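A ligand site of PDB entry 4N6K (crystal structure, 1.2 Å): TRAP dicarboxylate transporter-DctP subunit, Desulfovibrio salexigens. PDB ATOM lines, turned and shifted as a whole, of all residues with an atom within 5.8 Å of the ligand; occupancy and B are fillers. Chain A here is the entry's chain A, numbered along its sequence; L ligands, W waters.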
ATOM      1  N   VAL A  38     -19.569  -3.808  12.322  1.00  0.00           N
ATOM      2  CA  VAL A  38     -19.346  -5.242  12.179  1.00  0.00           C
ATOM      3  C   VAL A  38     -20.275  -6.090  13.024  1.00  0.00           C
ATOM      4  O   VAL A  38     -20.208  -7.313  12.960  1.00  0.00           O
ATOM      5  CB  VAL A  38     -17.868  -5.621  12.505  1.00  0.00           C
ATOM      6  CG1 VAL A  38     -16.922  -4.761  11.689  1.00  0.00           C
ATOM      7  CG2 VAL A  38     -17.575  -5.501  14.007  1.00  0.00           C
ATOM      8  N   PHE A  39     -21.070  -5.444  13.884  1.00  0.00           N
ATOM      9  CA  PHE A  39     -21.893  -6.113  14.898  1.00  0.00           C
ATOM     10  C   PHE A  39     -23.158  -6.760  14.323  1.00  0.00           C
ATOM     11  O   PHE A  39     -23.608  -6.448  13.222  1.00  0.00           O
ATOM     12  CB  PHE A  39     -22.247  -5.129  16.010  1.00  0.00           C
ATOM     13  CG  PHE A  39     -21.066  -4.645  16.828  1.00  0.00           C
ATOM     14  CD1 PHE A  39     -20.121  -3.770  16.292  1.00  0.00           C
ATOM     15  CD2 PHE A  39     -20.900  -5.051  18.141  1.00  0.00           C
ATOM     16  CE1 PHE A  39     -19.046  -3.322  17.040  1.00  0.00           C
ATOM     17  CE2 PHE A  39     -19.829  -4.593  18.899  1.00  0.00           C
ATOM     18  CZ  PHE A  39     -18.893  -3.747  18.335  1.00  0.00           C
ATOM     19  N   SER A  40     -23.724  -7.649  15.119  1.00  0.00           N
ATOM     20  CA  SER A  40     -24.880  -8.446  14.740  1.00  0.00           C
ATOM     21  C   SER A  40     -26.163  -7.793  15.238  1.00  0.00           C
ATOM     22  O   SER A  40     -26.149  -7.024  16.196  1.00  0.00           O
ATOM     23  CB  SER A  40     -24.749  -9.842  15.335  1.00  0.00           C
ATOM     24  OG  SER A  40     -23.763 -10.601  14.659  1.00  0.00           O
ATOM     25  N   GLU A  43     -27.012  -7.518  18.991  1.00  0.00           N
ATOM     26  CA  GLU A  43     -26.128  -6.759  19.869  1.00  0.00           C
ATOM     27  C   GLU A  43     -26.593  -5.330  20.027  1.00  0.00           C
ATOM     28  O   GLU A  43     -27.091  -4.703  19.088  1.00  0.00           O
ATOM     29  CB  GLU A  43     -24.711  -6.818  19.313  1.00  0.00           C
ATOM     30  CG  GLU A  43     -24.100  -8.194  19.435  1.00  0.00           C
ATOM     31  CD  GLU A  43     -22.714  -8.260  18.848  1.00  0.00           C
ATOM     32  OE1 GLU A  43     -22.574  -8.390  17.608  1.00  0.00           O
ATOM     33  OE2 GLU A  43     -21.746  -8.164  19.605  1.00  0.00           O
ATOM     34  N   TYR A  77     -14.132  -2.179   9.652  1.00  0.00           N
ATOM     35  CA  TYR A  77     -12.797  -2.091  10.216  1.00  0.00           C
ATOM     36  C   TYR A  77     -12.038  -0.955   9.503  1.00  0.00           C
ATOM     37  O   TYR A  77     -12.592   0.139   9.296  1.00  0.00           O
ATOM     38  CB  TYR A  77     -12.074  -3.431  10.146  1.00  0.00           C
ATOM     39  CG  TYR A  77     -12.724  -4.538  10.960  1.00  0.00           C
ATOM     40  CD1 TYR A  77     -12.782  -4.476  12.349  1.00  0.00           C
ATOM     41  CD2 TYR A  77     -13.282  -5.638  10.339  1.00  0.00           C
ATOM     42  CE1 TYR A  77     -13.335  -5.509  13.098  1.00  0.00           C
ATOM     43  CE2 TYR A  77     -13.848  -6.667  11.068  1.00  0.00           C
ATOM     44  CZ  TYR A  77     -13.888  -6.597  12.456  1.00  0.00           C
ATOM     45  OH  TYR A  77     -14.432  -7.652  13.157  1.00  0.00           O
ATOM     46  N   VAL A  93     -18.334   3.109  12.257  1.00  0.00           N
ATOM     47  CA  VAL A  93     -18.477   2.910  13.686  1.00  0.00           C
ATOM     48  C   VAL A  93     -17.578   1.754  14.066  1.00  0.00           C
ATOM     49  O   VAL A  93     -17.884   0.605  13.757  1.00  0.00           O
ATOM     50  CB  VAL A  93     -19.938   2.662  14.057  1.00  0.00           C
ATOM     51  CG1 VAL A  93     -20.105   2.400  15.541  1.00  0.00           C
ATOM     52  CG2 VAL A  93     -20.790   3.858  13.624  1.00  0.00           C
ATOM     53  N   GLU A  94     -16.433   2.075  14.647  1.00  0.00           N
ATOM     54  CA  GLU A  94     -15.351   1.132  14.932  1.00  0.00           C
ATOM     55  C   GLU A  94     -14.622   1.604  16.163  1.00  0.00           C
ATOM     56  O   GLU A  94     -14.683   2.780  16.512  1.00  0.00           O
ATOM     57  CB  GLU A  94     -14.337   1.056  13.797  1.00  0.00           C
ATOM     58  CG  GLU A  94     -14.927   0.685  12.450  1.00  0.00           C
ATOM     59  CD  GLU A  94     -15.421  -0.736  12.340  1.00  0.00           C
ATOM     60  OE1 GLU A  94     -15.143  -1.575  13.232  1.00  0.00           O
ATOM     61  OE2 GLU A  94     -16.108  -1.055  11.339  1.00  0.00           O
ATOM     62  N   ASP A  95     -13.906   0.699  16.829  1.00  0.00           N
ATOM     63  CA  ASP A  95     -13.135   1.151  17.981  1.00  0.00           C
ATOM     64  C   ASP A  95     -12.014   2.101  17.573  1.00  0.00           C
ATOM     65  O   ASP A  95     -11.606   2.153  16.413  1.00  0.00           O
ATOM     66  CB  ASP A  95     -12.655  -0.040  18.837  1.00  0.00           C
ATOM     67  CG  ASP A  95     -11.532  -0.827  18.217  1.00  0.00           C
ATOM     68  OD1 ASP A  95     -10.473  -0.244  18.020  1.00  0.00           O
ATOM     69  OD2 ASP A  95     -11.728  -2.040  17.956  1.00  0.00           O
ATOM     70  N   PHE A  98      -8.925   1.704  15.176  1.00  0.00           N
ATOM     71  CA  PHE A  98      -9.079   1.735  13.734  1.00  0.00           C
ATOM     72  C   PHE A  98      -8.905   3.123  13.137  1.00  0.00           C
ATOM     73  O   PHE A  98      -8.817   3.237  11.915  1.00  0.00           O
ATOM     74  CB  PHE A  98     -10.375   1.044  13.303  1.00  0.00           C
ATOM     75  CG  PHE A  98     -10.277  -0.441  13.493  1.00  0.00           C
ATOM     76  CD1 PHE A  98      -9.535  -1.184  12.590  1.00  0.00           C
ATOM     77  CD2 PHE A  98     -10.815  -1.076  14.590  1.00  0.00           C
ATOM     78  CE1 PHE A  98      -9.360  -2.552  12.791  1.00  0.00           C
ATOM     79  CE2 PHE A  98     -10.631  -2.439  14.792  1.00  0.00           C
ATOM     80  CZ  PHE A  98      -9.916  -3.173  13.887  1.00  0.00           C
ATOM     81  N   TYR A 110      -6.630   3.904  23.421  1.00  0.00           N
ATOM     82  CA  TYR A 110      -7.115   2.514  23.359  1.00  0.00           C
ATOM     83  C   TYR A 110      -6.079   1.540  23.907  1.00  0.00           C
ATOM     84  O   TYR A 110      -6.099   0.372  23.576  1.00  0.00           O
ATOM     85  CB  TYR A 110      -7.498   2.123  21.928  1.00  0.00           C
ATOM     86  CG  TYR A 110      -8.582   1.077  21.854  1.00  0.00           C
ATOM     87  CD1 TYR A 110      -9.868   1.365  22.282  1.00  0.00           C
ATOM     88  CD2 TYR A 110      -8.336  -0.213  21.357  1.00  0.00           C
ATOM     89  CE1 TYR A 110     -10.867   0.441  22.229  1.00  0.00           C
ATOM     90  CE2 TYR A 110      -9.352  -1.148  21.275  1.00  0.00           C
ATOM     91  CZ  TYR A 110     -10.616  -0.813  21.730  1.00  0.00           C
ATOM     92  OH  TYR A 110     -11.667  -1.696  21.672  1.00  0.00           O
ATOM     93  N   TYR A 151     -19.144  -1.236  24.458  1.00  0.00           N
ATOM     94  CA  TYR A 151     -19.783  -2.561  24.337  1.00  0.00           C
ATOM     95  C   TYR A 151     -19.188  -3.571  25.331  1.00  0.00           C
ATOM     96  O   TYR A 151     -19.564  -4.724  25.331  1.00  0.00           O
ATOM     97  CB  TYR A 151     -19.783  -3.080  22.886  1.00  0.00           C
ATOM     98  CG  TYR A 151     -18.415  -3.223  22.286  1.00  0.00           C
ATOM     99  CD1 TYR A 151     -17.652  -4.356  22.541  1.00  0.00           C
ATOM    100  CD2 TYR A 151     -17.840  -2.190  21.547  1.00  0.00           C
ATOM    101  CE1 TYR A 151     -16.385  -4.471  22.037  1.00  0.00           C
ATOM    102  CE2 TYR A 151     -16.563  -2.324  21.025  1.00  0.00           C
ATOM    103  CZ  TYR A 151     -15.836  -3.451  21.309  1.00  0.00           C
ATOM    104  OH  TYR A 151     -14.539  -3.580  20.847  1.00  0.00           O
ATOM    105  N   ARG A 154     -13.293  -6.336  27.406  1.00  0.00           N
ATOM    106  CA  ARG A 154     -12.990  -7.524  26.631  1.00  0.00           C
ATOM    107  C   ARG A 154     -12.181  -8.474  27.524  1.00  0.00           C
ATOM    108  O   ARG A 154     -11.206  -8.075  28.143  1.00  0.00           O
ATOM    109  CB  ARG A 154     -12.222  -7.163  25.362  1.00  0.00           C
ATOM    110  CG  ARG A 154     -13.013  -6.206  24.459  1.00  0.00           C
ATOM    111  CD  ARG A 154     -12.249  -5.744  23.222  1.00  0.00           C
ATOM    112  NE  ARG A 154     -11.954  -6.807  22.275  1.00  0.00           N
ATOM    113  CZ  ARG A 154     -12.496  -6.974  21.073  1.00  0.00           C
ATOM    114  NH1 ARG A 154     -13.446  -6.175  20.612  1.00  0.00           N
ATOM    115  NH2 ARG A 154     -12.101  -7.962  20.303  1.00  0.00           N
ATOM    116  N   ARG A 174      -7.707 -15.291  18.581  1.00  0.00           N
ATOM    117  CA  ARG A 174      -8.147 -14.327  17.595  1.00  0.00           C
ATOM    118  C   ARG A 174      -8.275 -12.956  18.227  1.00  0.00           C
ATOM    119  O   ARG A 174      -8.804 -12.804  19.337  1.00  0.00           O
ATOM    120  CB  ARG A 174      -9.471 -14.739  16.968  1.00  0.00           C
ATOM    121  CG  ARG A 174     -10.012 -13.728  15.956  1.00  0.00           C
ATOM    122  CD  ARG A 174     -10.905 -12.702  16.621  1.00  0.00           C
ATOM    123  NE  ARG A 174     -11.296 -11.630  15.707  1.00  0.00           N
ATOM    124  CZ  ARG A 174     -12.083 -10.630  16.035  1.00  0.00           C
ATOM    125  NH1 ARG A 174     -12.527 -10.512  17.290  1.00  0.00           N
ATOM    126  NH2 ARG A 174     -12.414  -9.729  15.127  1.00  0.00           N
ATOM    127  N   PRO A 176      -9.175  -8.648  16.652  1.00  0.00           N
ATOM    128  CA  PRO A 176      -9.374  -7.823  15.453  1.00  0.00           C
ATOM    129  C   PRO A 176      -8.035  -7.422  14.856  1.00  0.00           C
ATOM    130  O   PRO A 176      -7.000  -7.469  15.515  1.00  0.00           O
ATOM    131  CB  PRO A 176     -10.164  -6.626  15.985  1.00  0.00           C
ATOM    132  CG  PRO A 176     -10.785  -7.104  17.267  1.00  0.00           C
ATOM    133  CD  PRO A 176      -9.736  -7.990  17.848  1.00  0.00           C
ATOM    134  N   TYR A 181      -4.579  -4.422  19.212  1.00  0.00           N
ATOM    135  CA  TYR A 181      -4.969  -5.736  19.688  1.00  0.00           C
ATOM    136  C   TYR A 181      -3.837  -6.750  19.559  1.00  0.00           C
ATOM    137  O   TYR A 181      -3.604  -7.566  20.458  1.00  0.00           O
ATOM    138  CB  TYR A 181      -6.142  -6.260  18.884  1.00  0.00           C
ATOM    139  CG  TYR A 181      -7.438  -5.566  19.167  1.00  0.00           C
ATOM    140  CD1 TYR A 181      -8.161  -5.840  20.309  1.00  0.00           C
ATOM    141  CD2 TYR A 181      -7.978  -4.666  18.264  1.00  0.00           C
ATOM    142  CE1 TYR A 181      -9.376  -5.244  20.562  1.00  0.00           C
ATOM    143  CE2 TYR A 181      -9.193  -4.049  18.506  1.00  0.00           C
ATOM    144  CZ  TYR A 181      -9.885  -4.318  19.658  1.00  0.00           C
ATOM    145  OH  TYR A 181     -11.110  -3.750  19.903  1.00  0.00           O
ATOM    146  N   LEU A 195      -7.956 -11.394  12.829  1.00  0.00           N
ATOM    147  CA  LEU A 195      -8.940 -11.832  11.841  1.00  0.00           C
ATOM    148  C   LEU A 195     -10.159 -10.960  11.970  1.00  0.00           C
ATOM    149  O   LEU A 195     -10.573 -10.586  13.073  1.00  0.00           O
ATOM    150  CB  LEU A 195      -9.438 -13.251  12.123  1.00  0.00           C
ATOM    151  CG  LEU A 195      -8.387 -14.347  12.140  1.00  0.00           C
ATOM    152  CD1 LEU A 195      -8.961 -15.620  12.688  1.00  0.00           C
ATOM    153  CD2 LEU A 195      -7.817 -14.572  10.756  1.00  0.00           C
ATOM    154  N   PRO A 196     -10.827 -10.656  10.855  1.00  0.00           N
ATOM    155  CA  PRO A 196     -12.150 -10.026  10.962  1.00  0.00           C
ATOM    156  C   PRO A 196     -13.135 -10.974  11.634  1.00  0.00           C
ATOM    157  O   PRO A 196     -12.957 -12.196  11.603  1.00  0.00           O
ATOM    158  CB  PRO A 196     -12.529  -9.761   9.495  1.00  0.00           C
ATOM    159  CG  PRO A 196     -11.814 -10.882   8.734  1.00  0.00           C
ATOM    160  CD  PRO A 196     -10.495 -11.053   9.471  1.00  0.00           C
ATOM    161  N   TRP A 197     -14.193 -10.416  12.215  1.00  0.00           N
ATOM    162  CA  TRP A 197     -15.172 -11.235  12.917  1.00  0.00           C
ATOM    163  C   TRP A 197     -15.720 -12.343  12.046  1.00  0.00           C
ATOM    164  O   TRP A 197     -15.919 -13.454  12.518  1.00  0.00           O
ATOM    165  CB  TRP A 197     -16.333 -10.372  13.469  1.00  0.00           C
ATOM    166  CG  TRP A 197     -17.218 -11.174  14.342  1.00  0.00           C
ATOM    167  CD1 TRP A 197     -18.411 -11.705  14.020  1.00  0.00           C
ATOM    168  CD2 TRP A 197     -16.932 -11.598  15.670  1.00  0.00           C
ATOM    169  NE1 TRP A 197     -18.919 -12.429  15.074  1.00  0.00           N
ATOM    170  CE2 TRP A 197     -18.029 -12.366  16.113  1.00  0.00           C
ATOM    171  CE3 TRP A 197     -15.880 -11.371  16.557  1.00  0.00           C
ATOM    172  CZ2 TRP A 197     -18.083 -12.940  17.376  1.00  0.00           C
ATOM    173  CZ3 TRP A 197     -15.925 -11.919  17.808  1.00  0.00           C
ATOM    174  CH2 TRP A 197     -17.018 -12.698  18.222  1.00  0.00           C
ATOM    175  N   GLU A 213     -11.283 -13.166  22.254  1.00  0.00           N
ATOM    176  CA  GLU A 213     -11.455 -12.281  23.389  1.00  0.00           C
ATOM    177  C   GLU A 213     -12.541 -11.289  23.049  1.00  0.00           C
ATOM    178  O   GLU A 213     -12.697 -10.826  21.932  1.00  0.00           O
ATOM    179  CB  GLU A 213     -10.137 -11.614  23.793  1.00  0.00           C
ATOM    180  CG  GLU A 213      -9.294 -10.990  22.674  1.00  0.00           C
ATOM    181  CD  GLU A 213      -9.785  -9.646  22.196  1.00  0.00           C
ATOM    182  OE1 GLU A 213     -10.041  -8.782  23.070  1.00  0.00           O
ATOM    183  OE2 GLU A 213      -9.884  -9.467  20.964  1.00  0.00           O
ATOM    184  N   THR A 218     -20.715  -9.218  23.603  1.00  0.00           N
ATOM    185  CA  THR A 218     -20.346  -9.939  22.378  1.00  0.00           C
ATOM    186  C   THR A 218     -20.592 -11.449  22.533  1.00  0.00           C
ATOM    187  O   THR A 218     -21.143 -12.092  21.632  1.00  0.00           O
ATOM    188  CB  THR A 218     -18.863  -9.666  22.036  1.00  0.00           C
ATOM    189  OG1 THR A 218     -18.717  -8.280  21.680  1.00  0.00           O
ATOM    190  CG2 THR A 218     -18.370 -10.573  20.911  1.00  0.00           C
ATOM    191  N   THR A 222     -23.534 -12.863  19.999  1.00  0.00           N
ATOM    192  CA  THR A 222     -23.159 -13.641  18.839  1.00  0.00           C
ATOM    193  C   THR A 222     -23.117 -15.141  19.150  1.00  0.00           C
ATOM    194  O   THR A 222     -22.705 -15.937  18.314  1.00  0.00           O
ATOM    195  CB  THR A 222     -21.781 -13.227  18.292  1.00  0.00           C
ATOM    196  OG1 THR A 222     -20.755 -13.519  19.243  1.00  0.00           O
ATOM    197  CG2 THR A 222     -21.746 -11.751  17.915  1.00  0.00           C
ATOM    198  N   THR A 241     -14.996  -0.294  22.984  1.00  0.00           N
ATOM    199  CA  THR A 241     -15.858   0.861  22.745  1.00  0.00           C
ATOM    200  C   THR A 241     -15.729   1.250  21.279  1.00  0.00           C
ATOM    201  O   THR A 241     -14.643   1.184  20.696  1.00  0.00           O
ATOM    202  CB  THR A 241     -15.512   2.023  23.687  1.00  0.00           C
ATOM    203  OG1 THR A 241     -16.424   3.099  23.474  1.00  0.00           O
ATOM    204  CG2 THR A 241     -14.075   2.490  23.508  1.00  0.00           C
ATOM    205  N   CYS A 242     -16.865   1.623  20.679  1.00  0.00           N
ATOM    206  CA  CYS A 242     -16.863   2.209  19.344  1.00  0.00           C
ATOM    207  C   CYS A 242     -16.890   3.716  19.384  1.00  0.00           C
ATOM    208  O   CYS A 242     -17.569   4.327  20.220  1.00  0.00           O
ATOM    209  CB  CYS A 242     -18.066   1.747  18.524  1.00  0.00           C
ATOM    210  SG  CYS A 242     -18.008   0.020  18.021  1.00  0.00           S
HETATM  211  O1  LIG L   1     -14.180  -1.928  15.723  1.00  0.00           O
HETATM  212  C1  LIG L   1     -15.324  -2.573  16.275  1.00  0.00           C
HETATM  213  C2  LIG L   1     -15.009  -3.596  17.384  1.00  0.00           C
HETATM  214  O2  LIG L   1     -14.108  -3.102  18.325  1.00  0.00           O
HETATM  215  C3  LIG L   1     -14.473  -4.847  16.760  1.00  0.00           C
HETATM  216  O3  LIG L   1     -14.468  -5.945  17.718  1.00  0.00           O
HETATM  217  P1  LIG L   1     -14.678  -7.421  17.128  1.00  0.00           P
HETATM  218  O4  LIG L   1     -14.101  -7.519  15.753  1.00  0.00           O
HETATM  219  O5  LIG L   1     -14.144  -8.302  18.139  1.00  0.00           O
HETATM  220  O6  LIG L   1     -16.202  -7.582  16.977  1.00  0.00           O
HETATM  221  C4  LIG L   1     -17.025  -7.509  18.167  1.00  0.00           C
HETATM  222  C5  LIG L   1     -18.302  -8.321  18.018  1.00  0.00           C
HETATM  223  O7  LIG L   1     -19.181  -7.952  19.091  1.00  0.00           O
HETATM  224  C6  LIG L   1     -18.971  -8.233  16.630  1.00  0.00           C
HETATM  225  O8  LIG L   1     -20.211  -8.959  16.494  1.00  0.00           O
HETATM  226  O   HOH W   1     -17.801  -2.137  13.944  1.00  0.00           O
HETATM  227  O   HOH W   2     -14.914  -9.461  20.631  1.00  0.00           O
HETATM  228  O   HOH W   3     -21.255  -9.607  14.097  1.00  0.00           O
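Residues that only touch the ligand: Val 38, Phe 39, Ser 40, Phe 98, Pro 176, Trp 197 and Thr 222.
16 residues have an atom within 4 Å of the ligand: Val 38, Phe 39, Ser 40, Glu 43, Tyr 77, Glu 94, Asp 95, Phe 98, Tyr 151, Arg 154, Arg 174, Pro 176, Tyr 181, Trp 197, Thr 218 and Thr 222.
The guanidinium group (NH2) of Arg 174 sits at hydrogen-bond distance from the backbone carbonyl oxygen (O) of Leu 195 (2.9 Å).
OH of Tyr 181 sits at hydrogen-bond distance from OD2 of Asp 95 (2.7 Å).
The guanidinium group (NH2) of Arg 154 is in salt-bridge range of the side-chain carboxylate (OE2) of Glu 213 (2.8 Å).
The guanidinium group (NH1) of Arg 154 is in hydrogen-bond range of the side-chain hydroxyl (OH) of Tyr 181 (3.4 Å).
The backbone NH (N) of Tyr 77 sits at hydrogen-bond distance from the side-chain carboxylate (OE2) of Glu 94.
O of Thr 218 is in hydrogen-bond range of OG1 of Thr 222 (2.8 Å).
The backbone NH (N) of Trp 197 lies within hydrogen-bond range of the side-chain hydroxyl (OH) of Tyr 77 (2.9 Å).
The side-chain hydroxyl (OH) of Tyr 151 is in hydrogen-bond range of the guanidinium group (NH1) of Arg 154, 2.8 Å away.
Water W3 lies within hydrogen-bond range of O8 of the ligand (2.7 Å), OG of Ser 40 (2.8 Å) and O of Val 38 (2.8 Å).
Water W2 lies within hydrogen-bond range of O5 of the ligand (2.9 Å), O of Glu 213 (2.9 Å) and NH2 of Arg 154 (3.2 Å).
Water W1 lies within hydrogen-bond range of the backbone carbonyl oxygen of Val 93 (2.7 Å), the side-chain carboxylate of Glu 94 (2.8 Å) and the backbone NH of Val 38 (2.9 Å).
An oxygen (O4) of the ligand lies within salt-bridge range of the guanidinium group of Arg 174 (2.8 Å).
OH of Tyr 181 sits at hydrogen-bond distance from O2 of the ligand.
The guanidinium group (NH2) of Arg 154 is in salt-bridge range of an oxygen (O5) of the ligand (3.0 Å).
O2 of the ligand lies within hydrogen-bond range of OD2 of Asp 95 (2.6 Å).
O7 of the ligand lies within hydrogen-bond range of OE2 of Glu 43 (2.6 Å).
An oxygen (O2) of the ligand sits at hydrogen-bond distance from the side-chain hydroxyl (OH) of Tyr 151, 2.6 Å away.
An oxygen (O7) of the ligand is in hydrogen-bond range of the side-chain hydroxyl (OG1) of Thr 218 (2.7 Å).
The side-chain carboxylate (OE1) of Glu 94 lies within hydrogen-bond range of an oxygen (O1) of the ligand.
OH of Tyr 77 lies within hydrogen-bond range of O4 of the ligand, 2.6 Å away.
The backbone NH of Asp 95 is in hydrogen-bond range of an oxygen (O1) of the ligand (2.9 Å).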
